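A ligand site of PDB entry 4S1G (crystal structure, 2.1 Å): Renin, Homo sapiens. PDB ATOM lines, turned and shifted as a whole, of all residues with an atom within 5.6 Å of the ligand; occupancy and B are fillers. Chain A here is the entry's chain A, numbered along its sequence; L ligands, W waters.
A nitrogen (N2) of the ligand lies within hydrogen-bond range of the side-chain carboxylate (OD2) of Asp 38 (2.7 Å).
N3 of the ligand is in hydrogen-bond range of OD2 of Asp 226, 2.8 Å away.
The backbone carbonyl oxygen of Gly 228 is in hydrogen-bond range of a nitrogen (N4) of the ligand, at 3.0 Å.
O1 of the ligand lies within hydrogen-bond range of N of Thr 85, at 3.2 Å.
An oxygen (O1) of the ligand is in hydrogen-bond range of the side-chain hydroxyl (OG1) of Thr 85 (3.2 Å).
The backbone NH (N) of Gly 228 lies close to the side-chain carboxylate (OD1) of Asp 38, 3.3 Å away.
The side-chain carboxylate of Asp 38 sits at hydrogen-bond distance from the backbone NH of Gly 40, 3.0 Å away.
The side-chain carboxylate of Asp 38 sits at hydrogen-bond distance from the side-chain hydroxyl of Ser 41 (2.6 Å).
OD1 of Asp 226 sits at hydrogen-bond distance from N of Gly 228 (3.0 Å).
The side-chain carboxylate (OD1) of Asp 226 lies within hydrogen-bond range of the backbone NH (N) of Gly 40 (3.2 Å).
OH of Tyr 83 lies within hydrogen-bond range of NE1 of Trp 45 (3.0 Å).
OG of Ser 230 sits at hydrogen-bond distance from O of Thr 18 (2.7 Å).
The backbone carbonyl oxygen of Leu 121 lies within hydrogen-bond range of the side-chain amide nitrogen of Gln 19 (2.9 Å).
A fluorine (F1) of the ligand lies close to a ring nitrogen (NE2) of His 301 (3.3 Å).
Thr 18 touches the ligand (O to C24, 3.9 Å).
NE2 of Gln 19 touches C19 of the ligand, 3.8 Å away.
Gly 40 touches the ligand (CA to N3, 3.9 Å).
Tyr 83 touches the ligand.
Ser 84 touches the ligand.
Pro 118 touches the ligand.
Ala 122 touches the ligand (CB to C21, 3.9 Å).
Phe 124 touches the ligand.
Ala 229 touches the ligand (CA to C11, 3.8 Å).
Ser 230 touches the ligand.
CE of Met 303 touches F1 of the ligand (3.4 Å).
Hydrophobic or aromatic side chains within 4 Å of the ligand: Tyr 83, Pro 118, Ala 122, Phe 124, His 301 and Met 303.
16 residues have an atom within 4 Å of the ligand: Thr 18, Gln 19, Asp 38, Gly 40, Tyr 83, Ser 84, Thr 85, Pro 118, Ala 122, Phe 124, Asp 226, Gly 228, Ala 229, Ser 230, His 301 and Met 303.
Along chain A the residues within 4 Å of the ligand span positions 18 to 303.
Water W2 bridges the side-chain hydroxyl (OG) of Ser 230 (2.8 Å) and an oxygen (O2) of the ligand (3.0 Å).
Water W6 bridges the backbone NH of Ser 84 (3.3 Å) and an oxygen (O1) of the ligand (3.4 Å).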
ATOM      1  N   THR A  18      -0.866  15.555  16.203  1.00  0.00           N
ATOM      2  CA  THR A  18      -0.700  15.914  14.790  1.00  0.00           C
ATOM      3  C   THR A  18       0.758  16.052  14.390  1.00  0.00           C
ATOM      4  O   THR A  18       1.052  16.004  13.196  1.00  0.00           O
ATOM      5  CB  THR A  18      -1.490  17.205  14.441  1.00  0.00           C
ATOM      6  OG1 THR A  18      -1.014  18.281  15.260  1.00  0.00           O
ATOM      7  CG2 THR A  18      -2.969  17.072  14.601  1.00  0.00           C
ATOM      8  N   GLN A  19       1.677  16.318  15.342  1.00  0.00           N
ATOM      9  CA  GLN A  19       3.091  16.499  14.985  1.00  0.00           C
ATOM     10  C   GLN A  19       3.947  15.676  15.925  1.00  0.00           C
ATOM     11  O   GLN A  19       3.773  15.776  17.142  1.00  0.00           O
ATOM     12  CB  GLN A  19       3.503  17.983  15.032  1.00  0.00           C
ATOM     13  CG  GLN A  19       2.686  18.899  14.092  1.00  0.00           C
ATOM     14  CD  GLN A  19       2.957  20.370  14.299  1.00  0.00           C
ATOM     15  OE1 GLN A  19       4.074  20.772  14.622  1.00  0.00           O
ATOM     16  NE2 GLN A  19       1.932  21.199  14.126  1.00  0.00           N
ATOM     17  N   VAL A  36      10.691  16.381  12.025  1.00  0.00           N
ATOM     18  CA  VAL A  36       9.761  15.282  11.747  1.00  0.00           C
ATOM     19  C   VAL A  36      10.593  14.243  10.956  1.00  0.00           C
ATOM     20  O   VAL A  36      11.311  14.616  10.009  1.00  0.00           O
ATOM     21  CB  VAL A  36       8.502  15.740  10.959  1.00  0.00           C
ATOM     22  CG1 VAL A  36       7.653  14.528  10.526  1.00  0.00           C
ATOM     23  CG2 VAL A  36       7.660  16.690  11.786  1.00  0.00           C
ATOM     24  N   ASP A  38      10.281  11.631   8.478  1.00  0.00           N
ATOM     25  CA  ASP A  38       9.261  11.537   7.449  1.00  0.00           C
ATOM     26  C   ASP A  38       9.460  10.488   6.333  1.00  0.00           C
ATOM     27  O   ASP A  38      10.288  10.693   5.442  1.00  0.00           O
ATOM     28  CB  ASP A  38       9.143  12.946   6.839  1.00  0.00           C
ATOM     29  CG  ASP A  38       8.123  13.151   5.783  1.00  0.00           C
ATOM     30  OD1 ASP A  38       7.131  12.419   5.775  1.00  0.00           O
ATOM     31  OD2 ASP A  38       8.295  14.091   4.992  1.00  0.00           O
ATOM     32  N   GLY A  40       7.378  10.026   3.982  1.00  0.00           N
ATOM     33  CA  GLY A  40       6.796  10.673   2.807  1.00  0.00           C
ATOM     34  C   GLY A  40       7.712  11.578   2.017  1.00  0.00           C
ATOM     35  O   GLY A  40       7.276  12.187   1.037  1.00  0.00           O
ATOM     36  N   SER A  41       8.974  11.750   2.437  1.00  0.00           N
ATOM     37  CA  SER A  41       9.925  12.601   1.676  1.00  0.00           C
ATOM     38  C   SER A  41      11.314  12.027   1.849  1.00  0.00           C
ATOM     39  O   SER A  41      11.501  11.156   2.693  1.00  0.00           O
ATOM     40  CB  SER A  41       9.829  14.076   2.089  1.00  0.00           C
ATOM     41  OG  SER A  41      10.376  14.331   3.379  1.00  0.00           O
ATOM     42  N   TRP A  45      16.186  18.834   5.677  1.00  0.00           N
ATOM     43  CA  TRP A  45      16.262  20.289   5.626  1.00  0.00           C
ATOM     44  C   TRP A  45      15.965  20.905   6.970  1.00  0.00           C
ATOM     45  O   TRP A  45      15.170  20.360   7.735  1.00  0.00           O
ATOM     46  CB  TRP A  45      15.408  20.920   4.505  1.00  0.00           C
ATOM     47  CG  TRP A  45      13.919  20.783   4.697  1.00  0.00           C
ATOM     48  CD1 TRP A  45      13.103  19.855   4.103  1.00  0.00           C
ATOM     49  CD2 TRP A  45      13.060  21.656   5.450  1.00  0.00           C
ATOM     50  NE1 TRP A  45      11.795  20.095   4.453  1.00  0.00           N
ATOM     51  CE2 TRP A  45      11.739  21.197   5.265  1.00  0.00           C
ATOM     52  CE3 TRP A  45      13.288  22.795   6.245  1.00  0.00           C
ATOM     53  CZ2 TRP A  45      10.643  21.823   5.860  1.00  0.00           C
ATOM     54  CZ3 TRP A  45      12.195  23.429   6.829  1.00  0.00           C
ATOM     55  CH2 TRP A  45      10.890  22.931   6.645  1.00  0.00           C
ATOM     56  N   TYR A  83       5.972  20.141  -1.895  1.00  0.00           N
ATOM     57  CA  TYR A  83       5.233  19.127  -1.161  1.00  0.00           C
ATOM     58  C   TYR A  83       3.756  19.371  -1.315  1.00  0.00           C
ATOM     59  O   TYR A  83       3.360  20.454  -1.751  1.00  0.00           O
ATOM     60  CB  TYR A  83       5.570  19.238   0.335  1.00  0.00           C
ATOM     61  CG  TYR A  83       7.020  19.084   0.720  1.00  0.00           C
ATOM     62  CD1 TYR A  83       7.719  17.913   0.437  1.00  0.00           C
ATOM     63  CD2 TYR A  83       7.645  20.016   1.559  1.00  0.00           C
ATOM     64  CE1 TYR A  83       9.020  17.725   0.872  1.00  0.00           C
ATOM     65  CE2 TYR A  83       8.953  19.847   1.992  1.00  0.00           C
ATOM     66  CZ  TYR A  83       9.632  18.690   1.661  1.00  0.00           C
ATOM     67  OH  TYR A  83      10.907  18.484   2.130  1.00  0.00           O
ATOM     68  N   SER A  84       2.949  18.412  -0.828  1.00  0.00           N
ATOM     69  CA  SER A  84       1.486  18.509  -0.784  1.00  0.00           C
ATOM     70  C   SER A  84       1.050  19.702   0.080  1.00  0.00           C
ATOM     71  O   SER A  84      -0.008  20.279  -0.155  1.00  0.00           O
ATOM     72  CB  SER A  84       0.872  17.233  -0.233  1.00  0.00           C
ATOM     73  OG  SER A  84       1.298  16.128  -1.020  1.00  0.00           O
ATOM     74  N   THR A  85       1.834  20.011   1.136  1.00  0.00           N
ATOM     75  CA  THR A  85       1.519  21.118   2.051  1.00  0.00           C
ATOM     76  C   THR A  85       2.019  22.476   1.540  1.00  0.00           C
ATOM     77  O   THR A  85       1.694  23.508   2.117  1.00  0.00           O
ATOM     78  CB  THR A  85       2.075  20.853   3.471  1.00  0.00           C
ATOM     79  OG1 THR A  85       3.482  20.655   3.389  1.00  0.00           O
ATOM     80  CG2 THR A  85       1.403  19.722   4.163  1.00  0.00           C
ATOM     81  N   GLY A  86       2.836  22.446   0.522  1.00  0.00           N
ATOM     82  CA  GLY A  86       3.424  23.657  -0.033  1.00  0.00           C
ATOM     83  C   GLY A  86       4.881  23.494  -0.415  1.00  0.00           C
ATOM     84  O   GLY A  86       5.405  22.396  -0.358  1.00  0.00           O
ATOM     85  N   PRO A 118       2.246  26.434   5.708  1.00  0.00           N
ATOM     86  CA  PRO A 118       1.854  25.940   7.036  1.00  0.00           C
ATOM     87  C   PRO A 118       2.894  26.059   8.172  1.00  0.00           C
ATOM     88  O   PRO A 118       2.601  25.622   9.283  1.00  0.00           O
ATOM     89  CB  PRO A 118       1.663  24.450   6.740  1.00  0.00           C
ATOM     90  CG  PRO A 118       2.814  24.132   5.778  1.00  0.00           C
ATOM     91  CD  PRO A 118       2.944  25.384   4.925  1.00  0.00           C
ATOM     92  N   PHE A 119       4.088  26.608   7.913  1.00  0.00           N
ATOM     93  CA  PHE A 119       5.190  26.491   8.884  1.00  0.00           C
ATOM     94  C   PHE A 119       5.044  27.340  10.146  1.00  0.00           C
ATOM     95  O   PHE A 119       5.737  27.048  11.106  1.00  0.00           O
ATOM     96  CB  PHE A 119       6.561  26.675   8.189  1.00  0.00           C
ATOM     97  CG  PHE A 119       6.759  25.541   7.199  1.00  0.00           C
ATOM     98  CD1 PHE A 119       7.004  24.248   7.636  1.00  0.00           C
ATOM     99  CD2 PHE A 119       6.635  25.760   5.830  1.00  0.00           C
ATOM    100  CE1 PHE A 119       7.112  23.191   6.723  1.00  0.00           C
ATOM    101  CE2 PHE A 119       6.729  24.697   4.920  1.00  0.00           C
ATOM    102  CZ  PHE A 119       6.984  23.423   5.374  1.00  0.00           C
ATOM    103  N   LEU A 121       2.480  27.103  11.909  1.00  0.00           N
ATOM    104  CA  LEU A 121       1.690  26.136  12.697  1.00  0.00           C
ATOM    105  C   LEU A 121       2.571  24.962  13.159  1.00  0.00           C
ATOM    106  O   LEU A 121       2.133  24.116  13.947  1.00  0.00           O
ATOM    107  CB  LEU A 121       0.541  25.572  11.851  1.00  0.00           C
ATOM    108  CG  LEU A 121      -0.436  26.559  11.189  1.00  0.00           C
ATOM    109  CD1 LEU A 121      -1.182  25.890  10.038  1.00  0.00           C
ATOM    110  CD2 LEU A 121      -1.423  27.079  12.211  1.00  0.00           C
ATOM    111  N   ALA A 122       3.803  24.895  12.637  1.00  0.00           N
ATOM    112  CA  ALA A 122       4.706  23.806  12.970  1.00  0.00           C
ATOM    113  C   ALA A 122       5.458  24.056  14.266  1.00  0.00           C
ATOM    114  O   ALA A 122       6.093  25.097  14.432  1.00  0.00           O
ATOM    115  CB  ALA A 122       5.699  23.573  11.821  1.00  0.00           C
ATOM    116  N   PHE A 124       7.855  21.915  15.050  1.00  0.00           N
ATOM    117  CA  PHE A 124       9.173  21.440  14.661  1.00  0.00           C
ATOM    118  C   PHE A 124       9.827  22.494  13.784  1.00  0.00           C
ATOM    119  O   PHE A 124       9.120  23.366  13.257  1.00  0.00           O
ATOM    120  CB  PHE A 124       9.034  20.078  13.928  1.00  0.00           C
ATOM    121  CG  PHE A 124       8.121  20.106  12.717  1.00  0.00           C
ATOM    122  CD1 PHE A 124       6.762  19.878  12.837  1.00  0.00           C
ATOM    123  CD2 PHE A 124       8.629  20.365  11.439  1.00  0.00           C
ATOM    124  CE1 PHE A 124       5.924  19.908  11.718  1.00  0.00           C
ATOM    125  CE2 PHE A 124       7.791  20.394  10.319  1.00  0.00           C
ATOM    126  CZ  PHE A 124       6.449  20.151  10.459  1.00  0.00           C
ATOM    127  N   VAL A 127      12.842  18.874   8.692  1.00  0.00           N
ATOM    128  CA  VAL A 127      12.420  17.539   8.274  1.00  0.00           C
ATOM    129  C   VAL A 127      13.613  16.618   8.007  1.00  0.00           C
ATOM    130  O   VAL A 127      14.579  17.021   7.361  1.00  0.00           O
ATOM    131  CB  VAL A 127      11.492  17.621   7.012  1.00  0.00           C
ATOM    132  CG1 VAL A 127      11.140  16.222   6.458  1.00  0.00           C
ATOM    133  CG2 VAL A 127      10.221  18.424   7.295  1.00  0.00           C
ATOM    134  N   ASP A 226       2.845   7.160   5.511  1.00  0.00           N
ATOM    135  CA  ASP A 226       3.508   8.452   5.700  1.00  0.00           C
ATOM    136  C   ASP A 226       3.581   8.942   7.137  1.00  0.00           C
ATOM    137  O   ASP A 226       2.618   9.486   7.659  1.00  0.00           O
ATOM    138  CB  ASP A 226       2.811   9.496   4.788  1.00  0.00           C
ATOM    139  CG  ASP A 226       3.512  10.827   4.667  1.00  0.00           C
ATOM    140  OD1 ASP A 226       4.624  10.990   5.257  1.00  0.00           O
ATOM    141  OD2 ASP A 226       2.967  11.714   3.968  1.00  0.00           O
ATOM    142  N   GLY A 228       5.147  11.494   8.212  1.00  0.00           N
ATOM    143  CA  GLY A 228       5.099  12.958   8.186  1.00  0.00           C
ATOM    144  C   GLY A 228       3.714  13.556   7.949  1.00  0.00           C
ATOM    145  O   GLY A 228       3.578  14.782   7.897  1.00  0.00           O
ATOM    146  N   ALA A 229       2.672  12.709   7.793  1.00  0.00           N
ATOM    147  CA  ALA A 229       1.294  13.173   7.634  1.00  0.00           C
ATOM    148  C   ALA A 229       0.588  13.021   8.981  1.00  0.00           C
ATOM    149  O   ALA A 229       0.797  12.028   9.678  1.00  0.00           O
ATOM    150  CB  ALA A 229       0.581  12.317   6.580  1.00  0.00           C
ATOM    151  N   SER A 230      -0.261  13.990   9.354  1.00  0.00           N
ATOM    152  CA  SER A 230      -1.002  13.908  10.611  1.00  0.00           C
ATOM    153  C   SER A 230      -2.165  12.940  10.497  1.00  0.00           C
ATOM    154  O   SER A 230      -2.428  12.146  11.412  1.00  0.00           O
ATOM    155  CB  SER A 230      -1.554  15.280  11.006  1.00  0.00           C
ATOM    156  OG  SER A 230      -0.513  16.234  11.045  1.00  0.00           O
ATOM    157  N   SER A 233      -5.304  10.183   4.642  1.00  0.00           N
ATOM    158  CA  SER A 233      -5.894  10.903   3.524  1.00  0.00           C
ATOM    159  C   SER A 233      -6.306   9.954   2.397  1.00  0.00           C
ATOM    160  O   SER A 233      -5.715   8.891   2.222  1.00  0.00           O
ATOM    161  CB  SER A 233      -4.982  12.000   2.996  1.00  0.00           C
ATOM    162  OG  SER A 233      -3.880  11.469   2.294  1.00  0.00           O
ATOM    163  N   HIS A 301      -8.935  13.295   6.095  1.00  0.00           N
ATOM    164  CA  HIS A 301      -9.224  14.414   5.170  1.00  0.00           C
ATOM    165  C   HIS A 301      -8.895  14.034   3.728  1.00  0.00           C
ATOM    166  O   HIS A 301      -8.398  12.946   3.465  1.00  0.00           O
ATOM    167  CB  HIS A 301      -8.447  15.687   5.607  1.00  0.00           C
ATOM    168  CG  HIS A 301      -6.964  15.636   5.356  1.00  0.00           C
ATOM    169  ND1 HIS A 301      -6.265  16.757   4.985  1.00  0.00           N
ATOM    170  CD2 HIS A 301      -6.104  14.589   5.420  1.00  0.00           C
ATOM    171  CE1 HIS A 301      -5.013  16.377   4.842  1.00  0.00           C
ATOM    172  NE2 HIS A 301      -4.865  15.080   5.088  1.00  0.00           N
ATOM    173  N   MET A 303      -6.714  14.594   0.197  1.00  0.00           N
ATOM    174  CA  MET A 303      -5.447  15.073  -0.350  1.00  0.00           C
ATOM    175  C   MET A 303      -5.260  14.394  -1.677  1.00  0.00           C
ATOM    176  O   MET A 303      -5.136  13.163  -1.723  1.00  0.00           O
ATOM    177  CB  MET A 303      -4.247  14.852   0.625  1.00  0.00           C
ATOM    178  CG  MET A 303      -2.929  15.514   0.162  1.00  0.00           C
ATOM    179  SD  MET A 303      -2.953  17.342  -0.120  1.00  0.00           S
ATOM    180  CE  MET A 303      -3.749  17.914   1.400  1.00  0.00           C
HETATM  181  C1  LIG L   1       5.496  17.487   3.329  1.00  0.00           C
HETATM  182  C2  LIG L   1       4.128  16.885   3.149  1.00  0.00           C
HETATM  183  N1  LIG L   1       3.910  15.648   3.720  1.00  0.00           N
HETATM  184  C3  LIG L   1       4.962  14.923   4.277  1.00  0.00           C
HETATM  185  N2  LIG L   1       6.102  15.612   4.632  1.00  0.00           N
HETATM  186  C4  LIG L   1       6.234  17.046   4.585  1.00  0.00           C
HETATM  187  C5  LIG L   1       7.726  17.276   4.368  1.00  0.00           C
HETATM  188  C6  LIG L   1       5.696  17.728   5.855  1.00  0.00           C
HETATM  189  N3  LIG L   1       4.891  13.647   4.408  1.00  0.00           N
HETATM  190  C7  LIG L   1       2.590  15.051   3.563  1.00  0.00           C
HETATM  191  O1  LIG L   1       3.271  17.531   2.583  1.00  0.00           O
HETATM  192  C8  LIG L   1       6.121  17.014   7.144  1.00  0.00           C
HETATM  193  C9  LIG L   1       6.069  19.203   5.977  1.00  0.00           C
HETATM  194  C10 LIG L   1       1.489  15.728   4.317  1.00  0.00           C
HETATM  195  C11 LIG L   1       1.708  16.334   5.558  1.00  0.00           C
HETATM  196  C12 LIG L   1       0.655  16.940   6.229  1.00  0.00           C
HETATM  197  C13 LIG L   1      -0.605  16.937   5.678  1.00  0.00           C
HETATM  198  C14 LIG L   1      -0.813  16.359   4.435  1.00  0.00           C
HETATM  199  C15 LIG L   1       0.228  15.756   3.745  1.00  0.00           C
HETATM  200  F1  LIG L   1      -2.050  16.396   3.940  1.00  0.00           F
HETATM  201  C16 LIG L   1       0.800  17.553   7.569  1.00  0.00           C
HETATM  202  O2  LIG L   1      -0.089  18.266   8.022  1.00  0.00           O
HETATM  203  N4  LIG L   1       1.946  17.238   8.263  1.00  0.00           N
HETATM  204  C17 LIG L   1       2.192  17.840   9.571  1.00  0.00           C
HETATM  205  C18 LIG L   1       2.526  19.306   9.457  1.00  0.00           C
HETATM  206  C19 LIG L   1       2.167  20.172  10.482  1.00  0.00           C
HETATM  207  C20 LIG L   1       2.463  21.513  10.380  1.00  0.00           C
HETATM  208  C21 LIG L   1       3.131  22.018   9.269  1.00  0.00           C
HETATM  209  C22 LIG L   1       3.488  21.175   8.244  1.00  0.00           C
HETATM  210  C23 LIG L   1       3.174  19.818   8.339  1.00  0.00           C
HETATM  211  C24 LIG L   1       3.330  17.115  10.238  1.00  0.00           C
HETATM  212  O   HOH W   1      -2.315  15.173   7.644  1.00  0.00           O
HETATM  213  O   HOH W   2      -1.472  18.883  10.641  1.00  0.00           O
HETATM  214  O   HOH W   3      -1.553  12.944   2.882  1.00  0.00           O
HETATM  215  O   HOH W   4      -3.400  17.671   7.900  1.00  0.00           O
HETATM  216  O   HOH W   5      -3.325  19.582   4.270  1.00  0.00           O
HETATM  217  O   HOH W   6       4.681  15.711   0.029  1.00  0.00           O
HETATM  218  O   HOH W   7      -2.611  13.523   5.332  1.00  0.00           O
